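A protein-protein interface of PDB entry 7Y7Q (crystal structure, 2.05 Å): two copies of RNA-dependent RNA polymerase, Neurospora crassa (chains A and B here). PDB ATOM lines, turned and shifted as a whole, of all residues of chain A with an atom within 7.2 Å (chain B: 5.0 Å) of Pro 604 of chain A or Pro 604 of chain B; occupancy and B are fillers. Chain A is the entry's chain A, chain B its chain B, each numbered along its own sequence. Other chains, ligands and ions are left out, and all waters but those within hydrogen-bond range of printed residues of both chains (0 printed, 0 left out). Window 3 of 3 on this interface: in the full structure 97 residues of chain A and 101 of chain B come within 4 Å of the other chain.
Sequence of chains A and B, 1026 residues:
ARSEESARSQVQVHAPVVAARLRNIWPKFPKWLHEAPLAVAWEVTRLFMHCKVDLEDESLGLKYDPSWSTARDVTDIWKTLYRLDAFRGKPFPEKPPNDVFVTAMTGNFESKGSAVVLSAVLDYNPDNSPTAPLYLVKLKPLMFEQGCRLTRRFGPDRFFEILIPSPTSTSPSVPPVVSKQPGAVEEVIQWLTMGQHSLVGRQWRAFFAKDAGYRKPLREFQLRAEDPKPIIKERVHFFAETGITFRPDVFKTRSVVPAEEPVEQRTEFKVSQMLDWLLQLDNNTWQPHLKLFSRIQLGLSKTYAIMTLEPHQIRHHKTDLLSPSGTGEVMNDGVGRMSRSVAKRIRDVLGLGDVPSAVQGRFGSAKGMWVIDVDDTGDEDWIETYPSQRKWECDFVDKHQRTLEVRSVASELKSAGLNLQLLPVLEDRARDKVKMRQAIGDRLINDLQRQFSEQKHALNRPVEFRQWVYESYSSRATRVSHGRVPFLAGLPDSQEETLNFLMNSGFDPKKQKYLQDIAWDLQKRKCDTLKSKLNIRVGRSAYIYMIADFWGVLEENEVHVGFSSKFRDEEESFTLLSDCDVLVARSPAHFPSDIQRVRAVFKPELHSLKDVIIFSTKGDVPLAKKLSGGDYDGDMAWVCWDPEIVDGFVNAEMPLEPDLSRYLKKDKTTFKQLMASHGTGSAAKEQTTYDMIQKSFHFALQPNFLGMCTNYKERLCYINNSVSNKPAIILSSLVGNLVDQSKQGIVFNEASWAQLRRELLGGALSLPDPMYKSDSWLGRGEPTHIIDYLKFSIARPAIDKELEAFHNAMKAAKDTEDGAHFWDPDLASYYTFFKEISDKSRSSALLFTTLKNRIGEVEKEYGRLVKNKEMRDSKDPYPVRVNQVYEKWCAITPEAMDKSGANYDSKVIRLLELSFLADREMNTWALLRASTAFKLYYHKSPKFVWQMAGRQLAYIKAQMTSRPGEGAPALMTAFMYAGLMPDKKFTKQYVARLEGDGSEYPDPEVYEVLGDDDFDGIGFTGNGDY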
ATOM      1  N   VAL A 374       6.132  13.170  16.975  1.00  0.00           N
ATOM      2  CA  VAL A 374       5.239  14.329  16.702  1.00  0.00           C
ATOM      3  C   VAL A 374       4.020  14.284  17.628  1.00  0.00           C
ATOM      4  O   VAL A 374       3.396  15.319  17.816  1.00  0.00           O
ATOM      5  CB  VAL A 374       4.845  14.342  15.215  1.00  0.00           C
ATOM      6  CG1 VAL A 374       6.070  14.468  14.329  1.00  0.00           C
ATOM      7  CG2 VAL A 374       4.039  13.116  14.823  1.00  0.00           C
ATOM      8  N   VAL A 553       0.795   7.568   7.980  1.00  0.00           N
ATOM      9  CA  VAL A 553       0.058   8.523   7.161  1.00  0.00           C
ATOM     10  C   VAL A 553       0.489   8.497   5.700  1.00  0.00           C
ATOM     11  O   VAL A 553      -0.251   8.993   4.837  1.00  0.00           O
ATOM     12  CB  VAL A 553       0.205   9.951   7.717  1.00  0.00           C
ATOM     13  CG1 VAL A 553      -0.420  10.050   9.102  1.00  0.00           C
ATOM     14  CG2 VAL A 553       1.670  10.359   7.756  1.00  0.00           C
ATOM     15  N   HIS A 560       7.513  12.372   2.268  1.00  0.00           N
ATOM     16  CA  HIS A 560       7.241  13.677   2.858  1.00  0.00           C
ATOM     17  C   HIS A 560       8.563  14.406   3.055  1.00  0.00           C
ATOM     18  O   HIS A 560       9.473  13.875   3.700  1.00  0.00           O
ATOM     19  CB  HIS A 560       6.499  13.519   4.189  1.00  0.00           C
ATOM     20  CG  HIS A 560       6.336  14.795   4.959  1.00  0.00           C
ATOM     21  ND1 HIS A 560       5.120  15.427   5.098  1.00  0.00           N
ATOM     22  CD2 HIS A 560       7.229  15.541   5.652  1.00  0.00           C
ATOM     23  CE1 HIS A 560       5.272  16.513   5.835  1.00  0.00           C
ATOM     24  NE2 HIS A 560       6.542  16.606   6.185  1.00  0.00           N
ATOM     25  N   LEU A 576       8.620  23.289   1.467  1.00  0.00           N
ATOM     26  CA  LEU A 576       8.204  21.896   1.489  1.00  0.00           C
ATOM     27  C   LEU A 576       8.076  21.426   0.048  1.00  0.00           C
ATOM     28  O   LEU A 576       8.141  22.223  -0.891  1.00  0.00           O
ATOM     29  CB  LEU A 576       6.879  21.710   2.232  1.00  0.00           C
ATOM     30  CG  LEU A 576       5.717  22.557   1.707  1.00  0.00           C
ATOM     31  CD1 LEU A 576       4.907  21.773   0.679  1.00  0.00           C
ATOM     32  CD2 LEU A 576       4.829  23.024   2.847  1.00  0.00           C
ATOM     33  N   SER A 578       5.482  19.166  -2.490  1.00  0.00           N
ATOM     34  CA  SER A 578       4.131  18.635  -2.573  1.00  0.00           C
ATOM     35  C   SER A 578       3.668  18.670  -4.021  1.00  0.00           C
ATOM     36  O   SER A 578       4.100  19.518  -4.807  1.00  0.00           O
ATOM     37  CB  SER A 578       3.165  19.419  -1.679  1.00  0.00           C
ATOM     38  OG  SER A 578       1.893  18.798  -1.641  1.00  0.00           O
ATOM     39  N   ASP A 579       2.794  17.722  -4.364  1.00  0.00           N
ATOM     40  CA  ASP A 579       2.178  17.654  -5.688  1.00  0.00           C
ATOM     41  C   ASP A 579       3.230  17.570  -6.792  1.00  0.00           C
ATOM     42  O   ASP A 579       3.194  18.315  -7.774  1.00  0.00           O
ATOM     43  CB  ASP A 579       1.245  18.847  -5.917  1.00  0.00           C
ATOM     44  CG  ASP A 579       0.127  18.919  -4.895  1.00  0.00           C
ATOM     45  OD1 ASP A 579      -0.653  17.949  -4.796  1.00  0.00           O
ATOM     46  OD2 ASP A 579       0.030  19.949  -4.191  1.00  0.00           O
ATOM     47  N   VAL A 601       4.355  13.982  -1.098  1.00  0.00           N
ATOM     48  CA  VAL A 601       3.071  14.363  -0.522  1.00  0.00           C
ATOM     49  C   VAL A 601       3.340  14.935   0.861  1.00  0.00           C
ATOM     50  O   VAL A 601       3.940  14.264   1.707  1.00  0.00           O
ATOM     51  CB  VAL A 601       2.099  13.174  -0.435  1.00  0.00           C
ATOM     52  CG1 VAL A 601       0.790  13.608   0.209  1.00  0.00           C
ATOM     53  CG2 VAL A 601       1.854  12.583  -1.815  1.00  0.00           C
ATOM     54  N   PHE A 602       2.907  16.171   1.092  1.00  0.00           N
ATOM     55  CA  PHE A 602       3.107  16.817   2.382  1.00  0.00           C
ATOM     56  C   PHE A 602       1.968  16.432   3.318  1.00  0.00           C
ATOM     57  O   PHE A 602       0.796  16.677   3.012  1.00  0.00           O
ATOM     58  CB  PHE A 602       3.191  18.334   2.241  1.00  0.00           C
ATOM     59  CG  PHE A 602       3.643  19.026   3.492  1.00  0.00           C
ATOM     60  CD1 PHE A 602       4.994  19.154   3.775  1.00  0.00           C
ATOM     61  CD2 PHE A 602       2.718  19.529   4.398  1.00  0.00           C
ATOM     62  CE1 PHE A 602       5.418  19.783   4.931  1.00  0.00           C
ATOM     63  CE2 PHE A 602       3.135  20.157   5.556  1.00  0.00           C
ATOM     64  CZ  PHE A 602       4.489  20.284   5.822  1.00  0.00           C
ATOM     65  N   LYS A 603       2.316  15.833   4.455  1.00  0.00           N
ATOM     66  CA  LYS A 603       1.342  15.422   5.454  1.00  0.00           C
ATOM     67  C   LYS A 603       1.423  16.350   6.656  1.00  0.00           C
ATOM     68  O   LYS A 603       2.460  16.381   7.336  1.00  0.00           O
ATOM     69  CB  LYS A 603       1.580  13.973   5.878  1.00  0.00           C
ATOM     70  CG  LYS A 603       1.293  12.966   4.779  1.00  0.00           C
ATOM     71  CD  LYS A 603      -0.159  13.069   4.343  1.00  0.00           C
ATOM     72  CE  LYS A 603      -0.555  11.937   3.416  1.00  0.00           C
ATOM     73  NZ  LYS A 603      -2.029  11.712   3.450  1.00  0.00           N
ATOM     74  N   PRO A 604       0.370  17.118   6.948  1.00  0.00           N
ATOM     75  CA  PRO A 604       0.438  18.054   8.082  1.00  0.00           C
ATOM     76  C   PRO A 604       0.765  17.381   9.401  1.00  0.00           C
ATOM     77  O   PRO A 604       1.374  18.012  10.275  1.00  0.00           O
ATOM     78  CB  PRO A 604      -0.965  18.682   8.098  1.00  0.00           C
ATOM     79  CG  PRO A 604      -1.456  18.541   6.694  1.00  0.00           C
ATOM     80  CD  PRO A 604      -0.901  17.226   6.213  1.00  0.00           C
ATOM     81  N   GLU A 605       0.374  16.119   9.578  1.00  0.00           N
ATOM     82  CA  GLU A 605       0.737  15.390  10.789  1.00  0.00           C
ATOM     83  C   GLU A 605       2.245  15.362  11.005  1.00  0.00           C
ATOM     84  O   GLU A 605       2.711  15.304  12.149  1.00  0.00           O
ATOM     85  CB  GLU A 605       0.187  13.964  10.718  1.00  0.00           C
ATOM     86  CG  GLU A 605      -1.294  13.882  10.365  1.00  0.00           C
ATOM     87  CD  GLU A 605      -1.542  13.881   8.868  1.00  0.00           C
ATOM     88  OE1 GLU A 605      -1.022  14.787   8.181  1.00  0.00           O
ATOM     89  OE2 GLU A 605      -2.249  12.975   8.376  1.00  0.00           O
ATOM     90  N   LEU A 606       3.023  15.410   9.925  1.00  0.00           N
ATOM     91  CA  LEU A 606       4.476  15.313   9.991  1.00  0.00           C
ATOM     92  C   LEU A 606       5.166  16.672   9.907  1.00  0.00           C
ATOM     93  O   LEU A 606       6.396  16.724   9.792  1.00  0.00           O
ATOM     94  CB  LEU A 606       4.990  14.403   8.870  1.00  0.00           C
ATOM     95  CG  LEU A 606       4.308  13.041   8.735  1.00  0.00           C
ATOM     96  CD1 LEU A 606       4.871  12.268   7.553  1.00  0.00           C
ATOM     97  CD2 LEU A 606       4.458  12.240  10.016  1.00  0.00           C
ATOM     98  N   HIS A 607       4.409  17.770   9.984  1.00  0.00           N
ATOM     99  CA  HIS A 607       4.965  19.082   9.663  1.00  0.00           C
ATOM    100  C   HIS A 607       6.153  19.441  10.547  1.00  0.00           C
ATOM    101  O   HIS A 607       7.034  20.193  10.118  1.00  0.00           O
ATOM    102  CB  HIS A 607       3.883  20.157   9.779  1.00  0.00           C
ATOM    103  CG  HIS A 607       3.635  20.613  11.182  1.00  0.00           C
ATOM    104  ND1 HIS A 607       2.668  20.051  11.987  1.00  0.00           N
ATOM    105  CD2 HIS A 607       4.237  21.570  11.930  1.00  0.00           C
ATOM    106  CE1 HIS A 607       2.680  20.644  13.168  1.00  0.00           C
ATOM    107  NE2 HIS A 607       3.624  21.568  13.160  1.00  0.00           N
ATOM    108  N   SER A 608       6.196  18.932  11.780  1.00  0.00           N
ATOM    109  CA  SER A 608       7.299  19.286  12.666  1.00  0.00           C
ATOM    110  C   SER A 608       8.603  18.585  12.300  1.00  0.00           C
ATOM    111  O   SER A 608       9.648  18.931  12.862  1.00  0.00           O
ATOM    112  CB  SER A 608       6.931  18.976  14.119  1.00  0.00           C
ATOM    113  OG  SER A 608       6.766  17.582  14.320  1.00  0.00           O
ATOM    114  N   SER B 578       0.156  25.025  12.610  1.00  0.00           N
ATOM    115  CA  SER B 578      -0.761  23.861  12.527  1.00  0.00           C
ATOM    116  C   SER B 578      -1.033  23.287  13.917  1.00  0.00           C
ATOM    117  O   SER B 578      -0.139  23.380  14.764  1.00  0.00           O
ATOM    118  CB  SER B 578      -0.249  22.796  11.610  1.00  0.00           C
ATOM    119  OG  SER B 578      -1.313  21.991  11.132  1.00  0.00           O
ATOM    120  N   PHE B 602      -3.238  23.745   8.759  1.00  0.00           N
ATOM    121  CA  PHE B 602      -2.476  23.836   7.520  1.00  0.00           C
ATOM    122  C   PHE B 602      -3.092  22.911   6.479  1.00  0.00           C
ATOM    123  O   PHE B 602      -3.112  21.689   6.659  1.00  0.00           O
ATOM    124  CB  PHE B 602      -1.007  23.487   7.744  1.00  0.00           C
ATOM    125  CG  PHE B 602      -0.128  23.844   6.584  1.00  0.00           C
ATOM    126  CD1 PHE B 602       0.327  25.144   6.419  1.00  0.00           C
ATOM    127  CD2 PHE B 602       0.237  22.883   5.649  1.00  0.00           C
ATOM    128  CE1 PHE B 602       1.137  25.481   5.347  1.00  0.00           C
ATOM    129  CE2 PHE B 602       1.047  23.211   4.575  1.00  0.00           C
ATOM    130  CZ  PHE B 602       1.497  24.512   4.423  1.00  0.00           C
ATOM    131  N   LYS B 603      -3.589  23.500   5.393  1.00  0.00           N
ATOM    132  CA  LYS B 603      -4.179  22.743   4.302  1.00  0.00           C
ATOM    133  C   LYS B 603      -3.158  22.629   3.183  1.00  0.00           C
ATOM    134  O   LYS B 603      -2.798  23.653   2.584  1.00  0.00           O
ATOM    135  CB  LYS B 603      -5.448  23.428   3.798  1.00  0.00           C
ATOM    136  CG  LYS B 603      -6.481  23.696   4.877  1.00  0.00           C
ATOM    137  CD  LYS B 603      -7.154  22.410   5.329  1.00  0.00           C
ATOM    138  CE  LYS B 603      -8.286  22.697   6.304  1.00  0.00           C
ATOM    139  NZ  LYS B 603      -9.107  21.481   6.563  1.00  0.00           N
ATOM    140  N   PRO B 604      -2.657  21.431   2.873  1.00  0.00           N
ATOM    141  CA  PRO B 604      -1.660  21.318   1.795  1.00  0.00           C
ATOM    142  C   PRO B 604      -2.125  21.916   0.480  1.00  0.00           C
ATOM    143  O   PRO B 604      -1.288  22.316  -0.338  1.00  0.00           O
ATOM    144  CB  PRO B 604      -1.435  19.803   1.675  1.00  0.00           C
ATOM    145  CG  PRO B 604      -1.873  19.232   2.976  1.00  0.00           C
ATOM    146  CD  PRO B 604      -2.949  20.135   3.511  1.00  0.00           C
ATOM    147  N   GLU B 605      -3.439  21.985   0.254  1.00  0.00           N
ATOM    148  CA  GLU B 605      -3.968  22.604  -0.957  1.00  0.00           C
ATOM    149  C   GLU B 605      -3.498  24.049  -1.096  1.00  0.00           C
ATOM    150  O   GLU B 605      -3.239  24.524  -2.207  1.00  0.00           O
ATOM    151  CB  GLU B 605      -5.496  22.541  -0.944  1.00  0.00           C
ATOM    152  CG  GLU B 605      -6.058  21.145  -0.705  1.00  0.00           C
ATOM    153  CD  GLU B 605      -6.156  20.804   0.772  1.00  0.00           C
ATOM    154  OE1 GLU B 605      -5.098  20.672   1.423  1.00  0.00           O
ATOM    155  OE2 GLU B 605      -7.287  20.676   1.289  1.00  0.00           O
ATOM    156  N   LEU B 606      -3.365  24.759   0.025  1.00  0.00           N
ATOM    157  CA  LEU B 606      -3.001  26.171   0.034  1.00  0.00           C
ATOM    158  C   LEU B 606      -1.513  26.400   0.271  1.00  0.00           C
ATOM    159  O   LEU B 606      -1.101  27.540   0.509  1.00  0.00           O
ATOM    160  CB  LEU B 606      -3.816  26.909   1.098  1.00  0.00           C
ATOM    161  CG  LEU B 606      -5.325  26.666   1.057  1.00  0.00           C
ATOM    162  CD1 LEU B 606      -6.010  27.330   2.241  1.00  0.00           C
ATOM    163  CD2 LEU B 606      -5.910  27.172  -0.253  1.00  0.00           C
ATOM    164  N   HIS B 607      -0.697  25.345   0.187  1.00  0.00           N
ATOM    165  CA  HIS B 607       0.695  25.426   0.618  1.00  0.00           C
ATOM    166  C   HIS B 607       1.489  26.488  -0.135  1.00  0.00           C
ATOM    167  O   HIS B 607       2.484  26.994   0.394  1.00  0.00           O
ATOM    168  CB  HIS B 607       1.367  24.061   0.455  1.00  0.00           C
ATOM    169  CG  HIS B 607       1.794  23.762  -0.947  1.00  0.00           C
ATOM    170  ND1 HIS B 607       0.981  23.106  -1.848  1.00  0.00           N
ATOM    171  CD2 HIS B 607       2.946  24.029  -1.605  1.00  0.00           C
ATOM    172  CE1 HIS B 607       1.615  22.983  -3.000  1.00  0.00           C
ATOM    173  NE2 HIS B 607       2.810  23.535  -2.879  1.00  0.00           N
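Leu 576 of chain A touches Phe 602 of chain B. CD2 of His 607 of chain B touches CD1 of Leu 576 of chain A, 3.8 Å away. OD2 of Asp 579 of chain A touches CE1 of His 607 of chain B, at 3.6 Å. Phe 602 of chain A touches Phe 602 of chain B (CE2 to CE2, 3.8 Å). CG of Pro 604 of chain B touches O of Phe 602 of chain A, 3.7 Å away. Pro 604 of chain A touches Phe 602 of chain B (CG to O, 3.6 Å). Pro 604 of chain A touches Pro 604 of chain B (CG to CG, 3.8 Å). CE1 of His 607 of chain A touches CB of Ser 578 of chain B, at 3.95 Å.
Of the 14 printed residues of chain A, 5 touch a printed residue of chain B. Hydrophobic or aromatic side chains of chain A within 4 Å of the printed part of chain B: Leu 576, Phe 602, Pro 604 and His 607. Of the 7 printed residues of chain B, 4 touch a printed residue of chain A. Among the printed residues, no Asp or Glu carboxylate lies within 4 Å of a Lys or Arg side-chain nitrogen of the other chain.
The side-chain carboxylate of Asp 579 of chain A is in hydrogen-bond range of the side-chain hydroxyl of Ser 578 of chain A, 3.4 Å away. O of Pro 604 of chain A is in hydrogen-bond range of ND1 of His 607 of chain A. ND1 of His 607 of chain B sits at hydrogen-bond distance from O of Pro 604 of chain B (2.8 Å).
Phe 602 of chain B touches its own counterpart, Phe 602 of chain A. Phe 602 of chain A touches Pro 604 of chain B, and with the chains exchanged Pro 604 of chain A touches Phe 602 of chain B. Pro 604 of chain B touches its own counterpart, Pro 604 of chain A. His 607 of chain A touches Ser 578 of chain B, but with the chains exchanged Ser 578 of chain A does not touch His 607 of chain B (4.1 Å). Of the 8 pairs that touch across the chains among the printed residues, 4 have their exchanged pair printed and touching as well.
Of chain B, only Phe 602 (3.6 Å) and Pro 604 (3.8 Å) come within 4 Å of Pro 604 of chain A. Of the printed residues of chain A, Ser 578 of chain B touches His 607. Of the printed residues of chain A, His 607 of chain B touches Leu 576 (3.8 Å) and Asp 579 (3.6 Å). Printed residues of chain A within 4 Å of Phe 602 of chain B: Leu 576, Phe 602 and Pro 604. Of the printed residues of chain B, Phe 602 of chain A touches Phe 602 and Pro 604. Of the printed residues of chain B, His 607 of chain A touches Ser 578. Lys 603 of chain B touches none of the printed residues of chain A. The nearest residue of chain A that does not touch Pro 604 of chain B is Asp 579 of chain A (4.7 Å). The nearest printed residue of chain A that does not touch Phe 602 of chain B is His 607 of chain A (6.1 Å).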
